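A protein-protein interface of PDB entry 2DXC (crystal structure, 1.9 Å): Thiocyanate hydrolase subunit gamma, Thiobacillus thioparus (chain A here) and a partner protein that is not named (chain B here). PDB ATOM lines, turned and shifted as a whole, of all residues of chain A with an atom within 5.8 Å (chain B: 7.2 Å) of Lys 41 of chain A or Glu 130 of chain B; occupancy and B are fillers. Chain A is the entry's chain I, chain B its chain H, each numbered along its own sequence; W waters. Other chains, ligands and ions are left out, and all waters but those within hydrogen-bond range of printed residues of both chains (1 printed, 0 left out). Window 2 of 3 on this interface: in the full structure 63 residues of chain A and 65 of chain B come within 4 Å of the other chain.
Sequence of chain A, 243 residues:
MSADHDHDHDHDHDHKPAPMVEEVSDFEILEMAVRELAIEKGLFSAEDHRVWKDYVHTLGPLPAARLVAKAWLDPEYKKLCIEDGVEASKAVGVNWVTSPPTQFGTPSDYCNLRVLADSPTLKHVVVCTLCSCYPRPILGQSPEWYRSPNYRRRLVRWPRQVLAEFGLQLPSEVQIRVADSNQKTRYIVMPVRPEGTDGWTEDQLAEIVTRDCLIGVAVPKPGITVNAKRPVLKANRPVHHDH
OE2 of Glu 130 of chain B is in salt-bridge range of NZ of Lys 41 of chain A, 2.9 Å away. NZ of Lys 134 of chain B lies within salt-bridge range of OE2 of Glu 36 of chain A, 3.0 Å away. OE2 of Glu 40 of chain A is in salt-bridge range of NZ of Lys 134 of chain B, at 2.9 Å.
The backbone NH of Phe 125 of chain B sits at hydrogen-bond distance from the backbone carbonyl oxygen of Leu 120 of chain B, at 2.8 Å. The backbone carbonyl oxygen of Leu 120 of chain B lies within hydrogen-bond range of the backbone NH of Val 126 of chain B, at 3.1 Å. The side-chain carboxylate of Glu 130 of chain B lies within hydrogen-bond range of the backbone NH of Thr 127 of chain B. The backbone carbonyl oxygen (O) of Ala 38 of chain A sits at hydrogen-bond distance from the backbone NH (N) of Leu 43 of chain A (2.8 Å).
Among the printed residues, merely in contact across the chains: Leu 43 of chain A with Leu 120 of chain B (3.3 Å), Lys 41 of chain A with Phe 125 of chain B (3.5 Å), Leu 43 of chain A with Phe 125 of chain B (3.8 Å), Lys 41 of chain A with Val 126 of chain B (3.8 Å), Leu 37 of chain A with Lys 134 of chain B (3.9 Å) and Leu 37 of chain A with Leu 131 of chain B (3.9 Å).
Lys 41 of chain A touches just these residues of chain B: Phe 125 (3.5 Å), Val 126 (3.8 Å) and Glu 130 (2.9 Å). Glu 130 of chain B touches just one residue of chain A: Lys 41. Of the printed residues of chain A, Phe 125 of chain B touches Lys 41 and Leu 43. Printed residues of chain B within 4 Å of Glu 40 of chain A: Lys 134. Of the printed residues of chain B, Leu 43 of chain A touches Leu 120 and Phe 125. Of the printed residues of chain A, Leu 120 of chain B touches Leu 43. Of the printed residues of chain B, Glu 36 of chain A touches Lys 134 (3.0 Å). The nearest residue of chain B that does not touch Lys 41 of chain A is Thr 127 of chain B (6.0 Å). The nearest residue of chain A that does not touch Glu 130 of chain B is Leu 37 of chain A (4.2 Å).
Hydrophobic or aromatic side chains of chain B within 4 Å of the printed part of chain A: Leu 120, Phe 125, Val 126 and Leu 131. Printed residues of chain A that touch a printed residue of chain B: Glu 36, Leu 37, Glu 40, Lys 41 and Leu 43. Hydrophobic or aromatic side chains of chain A that line the printed part of chain B: Leu 37 and Leu 43. Among the printed residues, 9 pairs touch across the chains. Among the printed residues, Asp or Glu carboxylates within 4 Å of a Lys or Arg side-chain nitrogen of the other chain: Glu 36 of chain A with Lys 134 of chain B, Glu 40 of chain A with Lys 134 of chain B and Lys 41 of chain A with Glu 130 of chain B.
Water W1 lies within hydrogen-bond range of OE1 of Glu 40 of chain A (2.8 Å) and NZ of Lys 134 of chain B (3.5 Å).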
ATOM      1  N   GLU A  36     -30.352  -0.525  -7.585  1.00  0.00           N
ATOM      2  CA  GLU A  36     -29.546  -1.401  -6.741  1.00  0.00           C
ATOM      3  C   GLU A  36     -28.753  -0.589  -5.722  1.00  0.00           C
ATOM      4  O   GLU A  36     -28.660  -0.970  -4.557  1.00  0.00           O
ATOM      5  CB  GLU A  36     -28.601  -2.265  -7.587  1.00  0.00           C
ATOM      6  CG  GLU A  36     -29.316  -3.384  -8.342  1.00  0.00           C
ATOM      7  CD  GLU A  36     -28.376  -4.469  -8.850  1.00  0.00           C
ATOM      8  OE1 GLU A  36     -28.878  -5.441  -9.450  1.00  0.00           O
ATOM      9  OE2 GLU A  36     -27.144  -4.361  -8.648  1.00  0.00           O
ATOM     10  N   LEU A  37     -28.194   0.537  -6.153  1.00  0.00           N
ATOM     11  CA  LEU A  37     -27.424   1.380  -5.243  1.00  0.00           C
ATOM     12  C   LEU A  37     -28.301   1.967  -4.136  1.00  0.00           C
ATOM     13  O   LEU A  37     -27.904   1.993  -2.969  1.00  0.00           O
ATOM     14  CB  LEU A  37     -26.730   2.510  -6.016  1.00  0.00           C
ATOM     15  CG  LEU A  37     -25.508   2.111  -6.851  1.00  0.00           C
ATOM     16  CD1 LEU A  37     -25.100   3.264  -7.761  1.00  0.00           C
ATOM     17  CD2 LEU A  37     -24.360   1.733  -5.920  1.00  0.00           C
ATOM     18  N   ALA A  38     -29.491   2.435  -4.498  1.00  0.00           N
ATOM     19  CA  ALA A  38     -30.404   3.017  -3.519  1.00  0.00           C
ATOM     20  C   ALA A  38     -30.791   1.990  -2.451  1.00  0.00           C
ATOM     21  O   ALA A  38     -30.892   2.312  -1.266  1.00  0.00           O
ATOM     22  CB  ALA A  38     -31.654   3.540  -4.219  1.00  0.00           C
ATOM     23  N   ILE A  39     -31.014   0.753  -2.880  1.00  0.00           N
ATOM     24  CA  ILE A  39     -31.387  -0.305  -1.953  1.00  0.00           C
ATOM     25  C   ILE A  39     -30.184  -0.730  -1.113  1.00  0.00           C
ATOM     26  O   ILE A  39     -30.311  -0.955   0.087  1.00  0.00           O
ATOM     27  CB  ILE A  39     -31.958  -1.521  -2.714  1.00  0.00           C
ATOM     28  CG1 ILE A  39     -33.269  -1.121  -3.398  1.00  0.00           C
ATOM     29  CG2 ILE A  39     -32.202  -2.686  -1.750  1.00  0.00           C
ATOM     30  CD1 ILE A  39     -33.834  -2.178  -4.326  1.00  0.00           C
ATOM     31  N   GLU A  40     -29.017  -0.828  -1.740  1.00  0.00           N
ATOM     32  CA  GLU A  40     -27.807  -1.210  -1.018  1.00  0.00           C
ATOM     33  C   GLU A  40     -27.482  -0.184   0.070  1.00  0.00           C
ATOM     34  O   GLU A  40     -27.015  -0.541   1.153  1.00  0.00           O
ATOM     35  CB  GLU A  40     -26.625  -1.336  -1.990  1.00  0.00           C
ATOM     36  CG  GLU A  40     -26.697  -2.570  -2.890  1.00  0.00           C
ATOM     37  CD  GLU A  40     -25.668  -2.559  -4.012  1.00  0.00           C
ATOM     38  OE1 GLU A  40     -24.852  -1.615  -4.071  1.00  0.00           O
ATOM     39  OE2 GLU A  40     -25.678  -3.498  -4.838  1.00  0.00           O
ATOM     40  N   LYS A  41     -27.739   1.090  -0.220  1.00  0.00           N
ATOM     41  CA  LYS A  41     -27.470   2.166   0.733  1.00  0.00           C
ATOM     42  C   LYS A  41     -28.619   2.382   1.710  1.00  0.00           C
ATOM     43  O   LYS A  41     -28.551   3.248   2.580  1.00  0.00           O
ATOM     44  CB  LYS A  41     -27.183   3.474  -0.011  1.00  0.00           C
ATOM     45  CG  LYS A  41     -25.928   3.431  -0.859  1.00  0.00           C
ATOM     46  CD  LYS A  41     -24.701   3.093  -0.020  1.00  0.00           C
ATOM     47  CE  LYS A  41     -23.447   3.056  -0.882  1.00  0.00           C
ATOM     48  NZ  LYS A  41     -22.248   2.678  -0.094  1.00  0.00           N
ATOM     49  N   GLY A  42     -29.678   1.596   1.551  1.00  0.00           N
ATOM     50  CA  GLY A  42     -30.824   1.705   2.433  1.00  0.00           C
ATOM     51  C   GLY A  42     -31.623   2.989   2.315  1.00  0.00           C
ATOM     52  O   GLY A  42     -32.231   3.422   3.292  1.00  0.00           O
ATOM     53  N   LEU A  43     -31.634   3.607   1.137  1.00  0.00           N
ATOM     54  CA  LEU A  43     -32.390   4.844   0.947  1.00  0.00           C
ATOM     55  C   LEU A  43     -33.880   4.497   0.909  1.00  0.00           C
ATOM     56  O   LEU A  43     -34.717   5.216   1.458  1.00  0.00           O
ATOM     57  CB  LEU A  43     -31.927   5.542  -0.334  1.00  0.00           C
ATOM     58  CG  LEU A  43     -30.409   5.784  -0.332  1.00  0.00           C
ATOM     59  CD1 LEU A  43     -30.013   6.578  -1.554  1.00  0.00           C
ATOM     60  CD2 LEU A  43     -29.998   6.536   0.937  1.00  0.00           C
ATOM     61  N   LEU B 120     -28.334  10.953  -5.647  1.00  0.00           N
ATOM     62  CA  LEU B 120     -27.568  10.008  -4.839  1.00  0.00           C
ATOM     63  C   LEU B 120     -26.134  10.514  -4.669  1.00  0.00           C
ATOM     64  O   LEU B 120     -25.544  10.401  -3.592  1.00  0.00           O
ATOM     65  CB  LEU B 120     -27.532   8.625  -5.500  1.00  0.00           C
ATOM     66  CG  LEU B 120     -28.858   7.907  -5.764  1.00  0.00           C
ATOM     67  CD1 LEU B 120     -28.577   6.448  -6.107  1.00  0.00           C
ATOM     68  CD2 LEU B 120     -29.750   7.985  -4.542  1.00  0.00           C
ATOM     69  N   GLN B 124     -24.239  12.842  -1.491  1.00  0.00           N
ATOM     70  CA  GLN B 124     -23.240  11.884  -1.036  1.00  0.00           C
ATOM     71  C   GLN B 124     -23.727  10.566  -0.431  1.00  0.00           C
ATOM     72  O   GLN B 124     -23.106  10.040   0.491  1.00  0.00           O
ATOM     73  CB  GLN B 124     -22.291  12.592  -0.060  1.00  0.00           C
ATOM     74  CG  GLN B 124     -21.478  13.703  -0.729  1.00  0.00           C
ATOM     75  CD  GLN B 124     -20.795  14.636   0.264  1.00  0.00           C
ATOM     76  OE1 GLN B 124     -21.452  15.313   1.053  1.00  0.00           O
ATOM     77  NE2 GLN B 124     -19.469  14.676   0.222  1.00  0.00           N
ATOM     78  N   PHE B 125     -24.830  10.029  -0.939  1.00  0.00           N
ATOM     79  CA  PHE B 125     -25.322   8.750  -0.445  1.00  0.00           C
ATOM     80  C   PHE B 125     -24.494   7.674  -1.145  1.00  0.00           C
ATOM     81  O   PHE B 125     -24.365   6.548  -0.665  1.00  0.00           O
ATOM     82  CB  PHE B 125     -26.815   8.603  -0.737  1.00  0.00           C
ATOM     83  CG  PHE B 125     -27.675   9.515   0.089  1.00  0.00           C
ATOM     84  CD1 PHE B 125     -27.665   9.424   1.481  1.00  0.00           C
ATOM     85  CD2 PHE B 125     -28.466  10.487  -0.512  1.00  0.00           C
ATOM     86  CE1 PHE B 125     -28.430  10.292   2.264  1.00  0.00           C
ATOM     87  CE2 PHE B 125     -29.236  11.361   0.259  1.00  0.00           C
ATOM     88  CZ  PHE B 125     -29.218  11.265   1.649  1.00  0.00           C
ATOM     89  N   VAL B 126     -23.934   8.044  -2.292  1.00  0.00           N
ATOM     90  CA  VAL B 126     -23.052   7.168  -3.054  1.00  0.00           C
ATOM     91  C   VAL B 126     -21.976   8.081  -3.642  1.00  0.00           C
ATOM     92  O   VAL B 126     -22.246   9.250  -3.945  1.00  0.00           O
ATOM     93  CB  VAL B 126     -23.774   6.450  -4.228  1.00  0.00           C
ATOM     94  CG1 VAL B 126     -25.038   5.752  -3.732  1.00  0.00           C
ATOM     95  CG2 VAL B 126     -24.095   7.444  -5.329  1.00  0.00           C
ATOM     96  N   THR B 127     -20.756   7.573  -3.780  1.00  0.00           N
ATOM     97  CA  THR B 127     -19.698   8.377  -4.378  1.00  0.00           C
ATOM     98  C   THR B 127     -19.889   8.230  -5.885  1.00  0.00           C
ATOM     99  O   THR B 127     -20.534   7.284  -6.338  1.00  0.00           O
ATOM    100  CB  THR B 127     -18.296   7.844  -4.026  1.00  0.00           C
ATOM    101  OG1 THR B 127     -18.170   6.504  -4.513  1.00  0.00           O
ATOM    102  CG2 THR B 127     -18.065   7.870  -2.518  1.00  0.00           C
ATOM    103  N   LEU B 128     -19.350   9.157  -6.668  1.00  0.00           N
ATOM    104  CA  LEU B 128     -19.486   9.042  -8.113  1.00  0.00           C
ATOM    105  C   LEU B 128     -18.769   7.758  -8.530  1.00  0.00           C
ATOM    106  O   LEU B 128     -19.152   7.101  -9.491  1.00  0.00           O
ATOM    107  CB  LEU B 128     -18.858  10.245  -8.818  1.00  0.00           C
ATOM    108  CG  LEU B 128     -18.998  10.228 -10.343  1.00  0.00           C
ATOM    109  CD1 LEU B 128     -20.475  10.196 -10.721  1.00  0.00           C
ATOM    110  CD2 LEU B 128     -18.332  11.455 -10.938  1.00  0.00           C
ATOM    111  N   THR B 129     -17.724   7.405  -7.787  1.00  0.00           N
ATOM    112  CA  THR B 129     -16.953   6.199  -8.065  1.00  0.00           C
ATOM    113  C   THR B 129     -17.842   4.958  -7.950  1.00  0.00           C
ATOM    114  O   THR B 129     -17.769   4.055  -8.784  1.00  0.00           O
ATOM    115  CB  THR B 129     -15.760   6.081  -7.091  1.00  0.00           C
ATOM    116  OG1 THR B 129     -14.898   7.213  -7.266  1.00  0.00           O
ATOM    117  CG2 THR B 129     -14.966   4.801  -7.349  1.00  0.00           C
ATOM    118  N   GLU B 130     -18.686   4.917  -6.925  1.00  0.00           N
ATOM    119  CA  GLU B 130     -19.582   3.782  -6.744  1.00  0.00           C
ATOM    120  C   GLU B 130     -20.588   3.696  -7.893  1.00  0.00           C
ATOM    121  O   GLU B 130     -20.974   2.600  -8.302  1.00  0.00           O
ATOM    122  CB  GLU B 130     -20.320   3.892  -5.405  1.00  0.00           C
ATOM    123  CG  GLU B 130     -19.430   3.657  -4.187  1.00  0.00           C
ATOM    124  CD  GLU B 130     -20.180   3.837  -2.878  1.00  0.00           C
ATOM    125  OE1 GLU B 130     -20.772   4.919  -2.678  1.00  0.00           O
ATOM    126  OE2 GLU B 130     -20.179   2.902  -2.050  1.00  0.00           O
ATOM    127  N   LEU B 131     -21.010   4.846  -8.415  1.00  0.00           N
ATOM    128  CA  LEU B 131     -21.957   4.865  -9.527  1.00  0.00           C
ATOM    129  C   LEU B 131     -21.278   4.387 -10.808  1.00  0.00           C
ATOM    130  O   LEU B 131     -21.819   3.546 -11.525  1.00  0.00           O
ATOM    131  CB  LEU B 131     -22.526   6.274  -9.734  1.00  0.00           C
ATOM    132  CG  LEU B 131     -23.443   6.486 -10.947  1.00  0.00           C
ATOM    133  CD1 LEU B 131     -24.603   5.491 -10.917  1.00  0.00           C
ATOM    134  CD2 LEU B 131     -23.970   7.919 -10.934  1.00  0.00           C
ATOM    135  N   HIS B 132     -20.099   4.929 -11.102  1.00  0.00           N
ATOM    136  CA  HIS B 132     -19.350   4.522 -12.291  1.00  0.00           C
ATOM    137  C   HIS B 132     -19.058   3.021 -12.215  1.00  0.00           C
ATOM    138  O   HIS B 132     -19.220   2.296 -13.198  1.00  0.00           O
ATOM    139  CB  HIS B 132     -18.017   5.278 -12.384  1.00  0.00           C
ATOM    140  CG  HIS B 132     -18.152   6.719 -12.773  1.00  0.00           C
ATOM    141  ND1 HIS B 132     -17.078   7.583 -12.805  1.00  0.00           N
ATOM    142  CD2 HIS B 132     -19.229   7.441 -13.169  1.00  0.00           C
ATOM    143  CE1 HIS B 132     -17.488   8.775 -13.204  1.00  0.00           C
ATOM    144  NE2 HIS B 132     -18.788   8.715 -13.431  1.00  0.00           N
ATOM    145  N   ASN B 133     -18.620   2.564 -11.045  1.00  0.00           N
ATOM    146  CA  ASN B 133     -18.304   1.150 -10.851  1.00  0.00           C
ATOM    147  C   ASN B 133     -19.523   0.251 -11.048  1.00  0.00           C
ATOM    148  O   ASN B 133     -19.413  -0.836 -11.624  1.00  0.00           O
ATOM    149  CB  ASN B 133     -17.723   0.917  -9.452  1.00  0.00           C
ATOM    150  CG  ASN B 133     -16.296   1.425  -9.317  1.00  0.00           C
ATOM    151  OD1 ASN B 133     -15.691   1.889 -10.287  1.00  0.00           O
ATOM    152  ND2 ASN B 133     -15.748   1.334  -8.109  1.00  0.00           N
ATOM    153  N   LYS B 134     -20.681   0.701 -10.565  1.00  0.00           N
ATOM    154  CA  LYS B 134     -21.911  -0.074 -10.694  1.00  0.00           C
ATOM    155  C   LYS B 134     -22.334  -0.179 -12.161  1.00  0.00           C
ATOM    156  O   LYS B 134     -22.797  -1.227 -12.605  1.00  0.00           O
ATOM    157  CB  LYS B 134     -23.031   0.568  -9.862  1.00  0.00           C
ATOM    158  CG  LYS B 134     -24.402  -0.062 -10.071  1.00  0.00           C
ATOM    159  CD  LYS B 134     -24.481  -1.488  -9.543  1.00  0.00           C
ATOM    160  CE  LYS B 134     -24.567  -1.525  -8.021  1.00  0.00           C
ATOM    161  NZ  LYS B 134     -24.832  -2.914  -7.521  1.00  0.00           N
ATOM    162  N   ILE B 135     -22.173   0.904 -12.916  1.00  0.00           N
ATOM    163  CA  ILE B 135     -22.532   0.888 -14.330  1.00  0.00           C
ATOM    164  C   ILE B 135     -21.657  -0.117 -15.069  1.00  0.00           C
ATOM    165  O   ILE B 135     -22.147  -0.897 -15.882  1.00  0.00           O
ATOM    166  CB  ILE B 135     -22.361   2.282 -14.978  1.00  0.00           C
ATOM    167  CG1 ILE B 135     -23.364   3.264 -14.364  1.00  0.00           C
ATOM    168  CG2 ILE B 135     -22.572   2.194 -16.484  1.00  0.00           C
ATOM    169  CD1 ILE B 135     -24.836   2.863 -14.548  1.00  0.00           C
ATOM    170  N   VAL B 136     -20.358  -0.096 -14.782  1.00  0.00           N
ATOM    171  CA  VAL B 136     -19.405  -1.010 -15.417  1.00  0.00           C
ATOM    172  C   VAL B 136     -19.762  -2.468 -15.132  1.00  0.00           C
ATOM    173  O   VAL B 136     -19.717  -3.317 -16.021  1.00  0.00           O
ATOM    174  CB  VAL B 136     -17.962  -0.760 -14.902  1.00  0.00           C
ATOM    175  CG1 VAL B 136     -17.029  -1.848 -15.404  1.00  0.00           C
ATOM    176  CG2 VAL B 136     -17.473   0.604 -15.357  1.00  0.00           C
HETATM  177  O   HOH W   1     -22.454  -1.425  -5.498  1.00  0.00           O
